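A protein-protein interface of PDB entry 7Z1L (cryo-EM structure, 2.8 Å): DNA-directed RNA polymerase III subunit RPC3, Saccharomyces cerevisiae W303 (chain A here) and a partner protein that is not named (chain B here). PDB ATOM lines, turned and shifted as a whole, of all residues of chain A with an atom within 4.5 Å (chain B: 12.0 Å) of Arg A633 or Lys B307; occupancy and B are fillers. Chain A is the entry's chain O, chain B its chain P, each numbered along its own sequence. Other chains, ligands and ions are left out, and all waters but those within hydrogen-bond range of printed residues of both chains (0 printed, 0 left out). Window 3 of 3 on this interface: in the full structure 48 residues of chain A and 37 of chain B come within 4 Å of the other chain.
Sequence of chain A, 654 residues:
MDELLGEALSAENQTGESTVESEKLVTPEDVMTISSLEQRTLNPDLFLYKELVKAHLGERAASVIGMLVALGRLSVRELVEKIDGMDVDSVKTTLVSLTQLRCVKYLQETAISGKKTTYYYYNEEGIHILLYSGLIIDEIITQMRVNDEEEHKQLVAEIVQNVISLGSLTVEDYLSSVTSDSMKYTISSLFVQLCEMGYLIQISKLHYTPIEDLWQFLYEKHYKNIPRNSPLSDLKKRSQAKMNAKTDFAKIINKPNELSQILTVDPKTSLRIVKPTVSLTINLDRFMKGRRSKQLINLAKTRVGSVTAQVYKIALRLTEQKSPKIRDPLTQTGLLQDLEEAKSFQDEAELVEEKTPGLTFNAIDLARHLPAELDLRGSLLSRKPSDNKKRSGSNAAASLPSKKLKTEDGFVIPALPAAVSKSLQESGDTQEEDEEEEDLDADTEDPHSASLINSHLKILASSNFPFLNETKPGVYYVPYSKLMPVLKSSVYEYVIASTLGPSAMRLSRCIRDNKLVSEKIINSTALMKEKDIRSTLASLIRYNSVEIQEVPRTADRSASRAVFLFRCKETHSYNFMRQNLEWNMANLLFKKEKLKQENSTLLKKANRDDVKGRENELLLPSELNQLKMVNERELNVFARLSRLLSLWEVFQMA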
ATOM      1  N   LYS A 591       3.828  -5.081   7.538  1.00  0.00           N
ATOM      2  CA  LYS A 591       4.480  -4.204   8.508  1.00  0.00           C
ATOM      3  C   LYS A 591       3.552  -3.080   8.949  1.00  0.00           C
ATOM      4  O   LYS A 591       3.471  -2.761  10.144  1.00  0.00           O
ATOM      5  CB  LYS A 591       5.763  -3.627   7.913  1.00  0.00           C
ATOM      6  CG  LYS A 591       6.949  -4.568   7.931  1.00  0.00           C
ATOM      7  CD  LYS A 591       8.125  -3.959   7.189  1.00  0.00           C
ATOM      8  CE  LYS A 591       9.337  -4.868   7.222  1.00  0.00           C
ATOM      9  NZ  LYS A 591      10.357  -4.458   6.219  1.00  0.00           N
ATOM     10  N   LEU A 595       2.101  -2.461  12.750  1.00  0.00           N
ATOM     11  CA  LEU A 595       2.271  -1.190  13.450  1.00  0.00           C
ATOM     12  C   LEU A 595       0.931  -0.628  13.917  1.00  0.00           C
ATOM     13  O   LEU A 595       0.805  -0.153  15.057  1.00  0.00           O
ATOM     14  CB  LEU A 595       2.987  -0.193  12.542  1.00  0.00           C
ATOM     15  CG  LEU A 595       3.055   1.261  13.005  1.00  0.00           C
ATOM     16  CD1 LEU A 595       3.835   1.364  14.301  1.00  0.00           C
ATOM     17  CD2 LEU A 595       3.683   2.129  11.932  1.00  0.00           C
ATOM     18  N   MET A 629       4.423  10.170  14.602  1.00  0.00           N
ATOM     19  CA  MET A 629       5.341   9.161  14.082  1.00  0.00           C
ATOM     20  C   MET A 629       4.589   8.048  13.362  1.00  0.00           C
ATOM     21  O   MET A 629       5.002   7.609  12.281  1.00  0.00           O
ATOM     22  CB  MET A 629       6.197   8.610  15.228  1.00  0.00           C
ATOM     23  CG  MET A 629       7.269   7.582  14.852  1.00  0.00           C
ATOM     24  SD  MET A 629       6.708   5.874  14.663  1.00  0.00           S
ATOM     25  CE  MET A 629       6.404   5.432  16.372  1.00  0.00           C
ATOM     26  N   VAL A 630       3.473   7.590  13.939  1.00  0.00           N
ATOM     27  CA  VAL A 630       2.700   6.510  13.332  1.00  0.00           C
ATOM     28  C   VAL A 630       2.111   6.953  11.997  1.00  0.00           C
ATOM     29  O   VAL A 630       2.158   6.213  11.004  1.00  0.00           O
ATOM     30  CB  VAL A 630       1.610   6.029  14.307  1.00  0.00           C
ATOM     31  CG1 VAL A 630       0.495   5.316  13.563  1.00  0.00           C
ATOM     32  CG2 VAL A 630       2.212   5.117  15.363  1.00  0.00           C
ATOM     33  N   ASN A 631       1.554   8.167  11.947  1.00  0.00           N
ATOM     34  CA  ASN A 631       0.959   8.651  10.704  1.00  0.00           C
ATOM     35  C   ASN A 631       2.017   8.870   9.629  1.00  0.00           C
ATOM     36  O   ASN A 631       1.782   8.574   8.450  1.00  0.00           O
ATOM     37  CB  ASN A 631       0.173   9.933  10.965  1.00  0.00           C
ATOM     38  CG  ASN A 631      -1.271   9.660  11.327  1.00  0.00           C
ATOM     39  OD1 ASN A 631      -2.159   9.723  10.478  1.00  0.00           O
ATOM     40  ND2 ASN A 631      -1.513   9.347  12.592  1.00  0.00           N
ATOM     41  N   GLU A 632       3.192   9.380  10.014  1.00  0.00           N
ATOM     42  CA  GLU A 632       4.278   9.538   9.052  1.00  0.00           C
ATOM     43  C   GLU A 632       4.740   8.188   8.514  1.00  0.00           C
ATOM     44  O   GLU A 632       4.998   8.046   7.310  1.00  0.00           O
ATOM     45  CB  GLU A 632       5.442  10.288   9.699  1.00  0.00           C
ATOM     46  CG  GLU A 632       6.594  10.587   8.754  1.00  0.00           C
ATOM     47  CD  GLU A 632       6.207  11.541   7.642  1.00  0.00           C
ATOM     48  OE1 GLU A 632       5.392  12.452   7.894  1.00  0.00           O
ATOM     49  OE2 GLU A 632       6.717  11.377   6.513  1.00  0.00           O
ATOM     50  N   ARG A 633       4.839   7.184   9.390  1.00  0.00           N
ATOM     51  CA  ARG A 633       5.234   5.851   8.946  1.00  0.00           C
ATOM     52  C   ARG A 633       4.201   5.253   7.999  1.00  0.00           C
ATOM     53  O   ARG A 633       4.560   4.628   6.995  1.00  0.00           O
ATOM     54  CB  ARG A 633       5.452   4.941  10.155  1.00  0.00           C
ATOM     55  CG  ARG A 633       6.770   5.178  10.876  1.00  0.00           C
ATOM     56  CD  ARG A 633       7.349   3.882  11.414  1.00  0.00           C
ATOM     57  NE  ARG A 633       7.026   3.667  12.818  1.00  0.00           N
ATOM     58  CZ  ARG A 633       7.314   2.560  13.489  1.00  0.00           C
ATOM     59  NH1 ARG A 633       7.921   1.539  12.908  1.00  0.00           N
ATOM     60  NH2 ARG A 633       6.986   2.476  14.775  1.00  0.00           N
ATOM     61  N   GLU A 634       2.912   5.442   8.297  1.00  0.00           N
ATOM     62  CA  GLU A 634       1.861   4.933   7.419  1.00  0.00           C
ATOM     63  C   GLU A 634       1.891   5.619   6.058  1.00  0.00           C
ATOM     64  O   GLU A 634       1.712   4.967   5.018  1.00  0.00           O
ATOM     65  CB  GLU A 634       0.497   5.115   8.083  1.00  0.00           C
ATOM     66  CG  GLU A 634      -0.657   4.512   7.307  1.00  0.00           C
ATOM     67  CD  GLU A 634      -1.923   4.409   8.134  1.00  0.00           C
ATOM     68  OE1 GLU A 634      -1.853   4.624   9.363  1.00  0.00           O
ATOM     69  OE2 GLU A 634      -2.989   4.114   7.556  1.00  0.00           O
ATOM     70  N   LEU A 635       2.116   6.937   6.045  1.00  0.00           N
ATOM     71  CA  LEU A 635       2.220   7.666   4.785  1.00  0.00           C
ATOM     72  C   LEU A 635       3.404   7.183   3.958  1.00  0.00           C
ATOM     73  O   LEU A 635       3.287   7.001   2.739  1.00  0.00           O
ATOM     74  CB  LEU A 635       2.339   9.164   5.057  1.00  0.00           C
ATOM     75  CG  LEU A 635       1.084  10.014   4.879  1.00  0.00           C
ATOM     76  CD1 LEU A 635      -0.032   9.503   5.758  1.00  0.00           C
ATOM     77  CD2 LEU A 635       1.398  11.455   5.217  1.00  0.00           C
ATOM     78  N   ASN A 636       4.553   6.968   4.605  1.00  0.00           N
ATOM     79  CA  ASN A 636       5.717   6.452   3.890  1.00  0.00           C
ATOM     80  C   ASN A 636       5.457   5.050   3.353  1.00  0.00           C
ATOM     81  O   ASN A 636       5.880   4.717   2.237  1.00  0.00           O
ATOM     82  CB  ASN A 636       6.941   6.462   4.802  1.00  0.00           C
ATOM     83  CG  ASN A 636       7.430   7.862   5.103  1.00  0.00           C
ATOM     84  OD1 ASN A 636       7.474   8.719   4.221  1.00  0.00           O
ATOM     85  ND2 ASN A 636       7.805   8.103   6.354  1.00  0.00           N
ATOM     86  N   VAL A 637       4.754   4.220   4.129  1.00  0.00           N
ATOM     87  CA  VAL A 637       4.415   2.870   3.685  1.00  0.00           C
ATOM     88  C   VAL A 637       3.561   2.923   2.427  1.00  0.00           C
ATOM     89  O   VAL A 637       3.824   2.220   1.444  1.00  0.00           O
ATOM     90  CB  VAL A 637       3.701   2.100   4.811  1.00  0.00           C
ATOM     91  CG1 VAL A 637       2.900   0.938   4.244  1.00  0.00           C
ATOM     92  CG2 VAL A 637       4.698   1.600   5.822  1.00  0.00           C
ATOM     93  N   PRO B 301      18.689   8.140  -0.695  1.00  0.00           N
ATOM     94  CA  PRO B 301      18.595   6.961   0.173  1.00  0.00           C
ATOM     95  C   PRO B 301      17.783   7.258   1.423  1.00  0.00           C
ATOM     96  O   PRO B 301      17.729   8.393   1.902  1.00  0.00           O
ATOM     97  CB  PRO B 301      20.058   6.651   0.515  1.00  0.00           C
ATOM     98  CG  PRO B 301      20.861   7.348  -0.536  1.00  0.00           C
ATOM     99  CD  PRO B 301      20.082   8.573  -0.889  1.00  0.00           C
ATOM    100  N   ALA B 302      17.141   6.219   1.947  1.00  0.00           N
ATOM    101  CA  ALA B 302      16.298   6.373   3.123  1.00  0.00           C
ATOM    102  C   ALA B 302      17.137   6.636   4.367  1.00  0.00           C
ATOM    103  O   ALA B 302      18.307   6.255   4.451  1.00  0.00           O
ATOM    104  CB  ALA B 302      15.442   5.128   3.338  1.00  0.00           C
ATOM    105  N   SER B 303      16.519   7.301   5.339  1.00  0.00           N
ATOM    106  CA  SER B 303      17.167   7.533   6.619  1.00  0.00           C
ATOM    107  C   SER B 303      17.328   6.222   7.378  1.00  0.00           C
ATOM    108  O   SER B 303      16.553   5.277   7.205  1.00  0.00           O
ATOM    109  CB  SER B 303      16.358   8.525   7.455  1.00  0.00           C
ATOM    110  OG  SER B 303      16.804   8.540   8.799  1.00  0.00           O
ATOM    111  N   LYS B 304      18.354   6.169   8.222  1.00  0.00           N
ATOM    112  CA  LYS B 304      18.598   4.981   9.021  1.00  0.00           C
ATOM    113  C   LYS B 304      17.541   4.850  10.116  1.00  0.00           C
ATOM    114  O   LYS B 304      16.771   5.776  10.393  1.00  0.00           O
ATOM    115  CB  LYS B 304      19.999   5.021   9.628  1.00  0.00           C
ATOM    116  CG  LYS B 304      21.115   5.040   8.596  1.00  0.00           C
ATOM    117  CD  LYS B 304      21.067   3.804   7.712  1.00  0.00           C
ATOM    118  CE  LYS B 304      21.393   2.546   8.500  1.00  0.00           C
ATOM    119  NZ  LYS B 304      22.793   2.554   9.006  1.00  0.00           N
ATOM    120  N   HIS B 305      17.514   3.666  10.735  1.00  0.00           N
ATOM    121  CA  HIS B 305      16.532   3.302  11.763  1.00  0.00           C
ATOM    122  C   HIS B 305      15.100   3.420  11.249  1.00  0.00           C
ATOM    123  O   HIS B 305      14.193   3.807  11.989  1.00  0.00           O
ATOM    124  CB  HIS B 305      16.715   4.130  13.040  1.00  0.00           C
ATOM    125  CG  HIS B 305      18.084   4.029  13.636  1.00  0.00           C
ATOM    126  ND1 HIS B 305      19.173   4.694  13.116  1.00  0.00           N
ATOM    127  CD2 HIS B 305      18.542   3.339  14.708  1.00  0.00           C
ATOM    128  CE1 HIS B 305      20.243   4.419  13.841  1.00  0.00           C
ATOM    129  NE2 HIS B 305      19.886   3.599  14.813  1.00  0.00           N
ATOM    130  N   ASP B 306      14.887   3.089   9.979  1.00  0.00           N
ATOM    131  CA  ASP B 306      13.563   3.075   9.371  1.00  0.00           C
ATOM    132  C   ASP B 306      13.161   1.626   9.137  1.00  0.00           C
ATOM    133  O   ASP B 306      13.849   0.898   8.413  1.00  0.00           O
ATOM    134  CB  ASP B 306      13.550   3.862   8.060  1.00  0.00           C
ATOM    135  CG  ASP B 306      12.147   4.138   7.560  1.00  0.00           C
ATOM    136  OD1 ASP B 306      12.005   4.587   6.404  1.00  0.00           O
ATOM    137  OD2 ASP B 306      11.186   3.908   8.323  1.00  0.00           O
ATOM    138  N   LYS B 307      12.052   1.211   9.751  1.00  0.00           N
ATOM    139  CA  LYS B 307      11.655  -0.192   9.690  1.00  0.00           C
ATOM    140  C   LYS B 307      11.080  -0.553   8.327  1.00  0.00           C
ATOM    141  O   LYS B 307      11.387  -1.621   7.782  1.00  0.00           O
ATOM    142  CB  LYS B 307      10.643  -0.500  10.793  1.00  0.00           C
ATOM    143  CG  LYS B 307      11.256  -0.736  12.163  1.00  0.00           C
ATOM    144  CD  LYS B 307      11.340   0.554  12.961  1.00  0.00           C
ATOM    145  CE  LYS B 307      11.663   0.282  14.420  1.00  0.00           C
ATOM    146  NZ  LYS B 307      11.717   1.540  15.214  1.00  0.00           N
ATOM    147  N   GLU B 308      10.248   0.317   7.759  1.00  0.00           N
ATOM    148  CA  GLU B 308       9.501  -0.010   6.544  1.00  0.00           C
ATOM    149  C   GLU B 308      10.248   0.511   5.315  1.00  0.00           C
ATOM    150  O   GLU B 308       9.791   1.389   4.582  1.00  0.00           O
ATOM    151  CB  GLU B 308       8.089   0.550   6.623  1.00  0.00           C
ATOM    152  CG  GLU B 308       7.316   0.101   7.850  1.00  0.00           C
ATOM    153  CD  GLU B 308       7.459   1.067   9.005  1.00  0.00           C
ATOM    154  OE1 GLU B 308       8.145   2.095   8.832  1.00  0.00           O
ATOM    155  OE2 GLU B 308       6.889   0.800  10.083  1.00  0.00           O
ATOM    156  N   VAL B 309      11.424  -0.068   5.100  1.00  0.00           N
ATOM    157  CA  VAL B 309      12.258   0.224   3.943  1.00  0.00           C
ATOM    158  C   VAL B 309      12.369  -1.048   3.107  1.00  0.00           C
ATOM    159  O   VAL B 309      12.481  -2.151   3.655  1.00  0.00           O
ATOM    160  CB  VAL B 309      13.633   0.785   4.364  1.00  0.00           C
ATOM    161  CG1 VAL B 309      14.443  -0.230   5.141  1.00  0.00           C
ATOM    162  CG2 VAL B 309      14.412   1.266   3.156  1.00  0.00           C
ATOM    163  N   VAL B 310      12.270  -0.897   1.790  1.00  0.00           N
ATOM    164  CA  VAL B 310      12.126  -2.028   0.880  1.00  0.00           C
ATOM    165  C   VAL B 310      13.483  -2.377   0.290  1.00  0.00           C
ATOM    166  O   VAL B 310      14.185  -1.506  -0.238  1.00  0.00           O
ATOM    167  CB  VAL B 310      11.109  -1.708  -0.228  1.00  0.00           C
ATOM    168  CG1 VAL B 310      11.117  -2.788  -1.296  1.00  0.00           C
ATOM    169  CG2 VAL B 310       9.720  -1.541   0.357  1.00  0.00           C
ATOM    170  N   TYR B 311      13.857  -3.653   0.375  1.00  0.00           N
ATOM    171  CA  TYR B 311      15.125  -4.144  -0.145  1.00  0.00           C
ATOM    172  C   TYR B 311      14.876  -5.073  -1.321  1.00  0.00           C
ATOM    173  O   TYR B 311      13.983  -5.924  -1.270  1.00  0.00           O
ATOM    174  CB  TYR B 311      15.919  -4.889   0.926  1.00  0.00           C
ATOM    175  CG  TYR B 311      16.421  -4.027   2.056  1.00  0.00           C
ATOM    176  CD1 TYR B 311      17.638  -3.368   1.964  1.00  0.00           C
ATOM    177  CD2 TYR B 311      15.691  -3.897   3.225  1.00  0.00           C
ATOM    178  CE1 TYR B 311      18.104  -2.587   2.999  1.00  0.00           C
ATOM    179  CE2 TYR B 311      16.151  -3.126   4.265  1.00  0.00           C
ATOM    180  CZ  TYR B 311      17.355  -2.468   4.148  1.00  0.00           C
ATOM    181  OH  TYR B 311      17.813  -1.693   5.186  1.00  0.00           O
ATOM    182  N   PHE B 312      15.673  -4.909  -2.379  1.00  0.00           N
ATOM    183  CA  PHE B 312      15.636  -5.848  -3.493  1.00  0.00           C
ATOM    184  C   PHE B 312      16.210  -7.203  -3.102  1.00  0.00           C
ATOM    185  O   PHE B 312      15.729  -8.240  -3.571  1.00  0.00           O
ATOM    186  CB  PHE B 312      16.399  -5.267  -4.682  1.00  0.00           C
ATOM    187  CG  PHE B 312      16.447  -6.171  -5.878  1.00  0.00           C
ATOM    188  CD1 PHE B 312      15.303  -6.432  -6.612  1.00  0.00           C
ATOM    189  CD2 PHE B 312      17.640  -6.747  -6.276  1.00  0.00           C
ATOM    190  CE1 PHE B 312      15.347  -7.260  -7.715  1.00  0.00           C
ATOM    191  CE2 PHE B 312      17.692  -7.574  -7.379  1.00  0.00           C
ATOM    192  CZ  PHE B 312      16.543  -7.830  -8.100  1.00  0.00           C
ATOM    193  N   GLU B 314      15.987  -8.751  -0.339  1.00  0.00           N
ATOM    194  CA  GLU B 314      15.130  -9.512   0.554  1.00  0.00           C
ATOM    195  C   GLU B 314      14.271 -10.479  -0.262  1.00  0.00           C
ATOM    196  O   GLU B 314      14.157 -10.359  -1.486  1.00  0.00           O
ATOM    197  CB  GLU B 314      14.276  -8.552   1.387  1.00  0.00           C
ATOM    198  CG  GLU B 314      13.655  -9.135   2.641  1.00  0.00           C
ATOM    199  CD  GLU B 314      12.987  -8.077   3.493  1.00  0.00           C
ATOM    200  OE1 GLU B 314      12.989  -6.897   3.087  1.00  0.00           O
ATOM    201  OE2 GLU B 314      12.471  -8.419   4.575  1.00  0.00           O
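NZ of Lys A591 is in hydrogen-bond range of O of Lys B307 (3.4 Å).
NH1 of Arg A633 lies within salt-bridge range of OE2 of Glu B308, at 3.1 Å.
The side-chain sulfur of Met A629 lies within hydrogen-bond range of the guanidinium group of Arg A633 (2.9 Å).
OE2 of Glu B308 touches CD2 of Leu A595, at 3.9 Å.
Arg A633 touches Lys B307 (NH1 to CD, 3.6 Å).
Glu B308 touches Val A637 (CG to CG2, 3.6 Å).
Of chain B, only Lys B307 and Glu B308 come within 4 Å of Arg A633.
Of chain A, only Lys A591 (3.4 Å) and Arg A633 (3.6 Å) come within 4 Å of Lys B307.
Leu A595 touches one residue of chain B.
No residue of chain B comes within 4 Å of Met A629.
No residue of chain B comes within 4 Å of Asn A631.
No residue of chain B comes within 4 Å of Glu A632.
No residue of chain B comes within 4 Å of Glu A634.
No residue of chain B comes within 4 Å of Asn A636.
Of chain B, only Glu B308 comes within 4 Å of Val A637.
Printed residues of chain A within 4 Å of Glu B308: Leu A595, Arg A633 and Val A637.
Printed residues of chain B within 4 Å of Lys A591: Lys B307 (3.4 Å).
Pro B301 touches none of the printed residues of chain A.
Glu B314 touches none of the printed residues of chain A.
The nearest residue of chain B that does not touch Arg A633 is Asp B306 (4.9 Å).
The nearest printed residue of chain A that does not touch Lys B307 is Met A629 (6.6 Å).
Of the 11 printed residues of chain A, 4 touch a printed residue of chain B.
Printed residues of chain A that touch a printed residue of chain B: Lys A591, Leu A595, Arg A633 and Val A637.
Along chain A the printed residues that touch a printed residue of chain B span positions 591 to 637.
Among the printed residues, 5 pairs touch across the chains.
Among the printed residues, Asp or Glu carboxylates within 4 Å of a Lys or Arg side-chain nitrogen of the other chain: Arg A633 with Glu B308 (3.1 Å).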
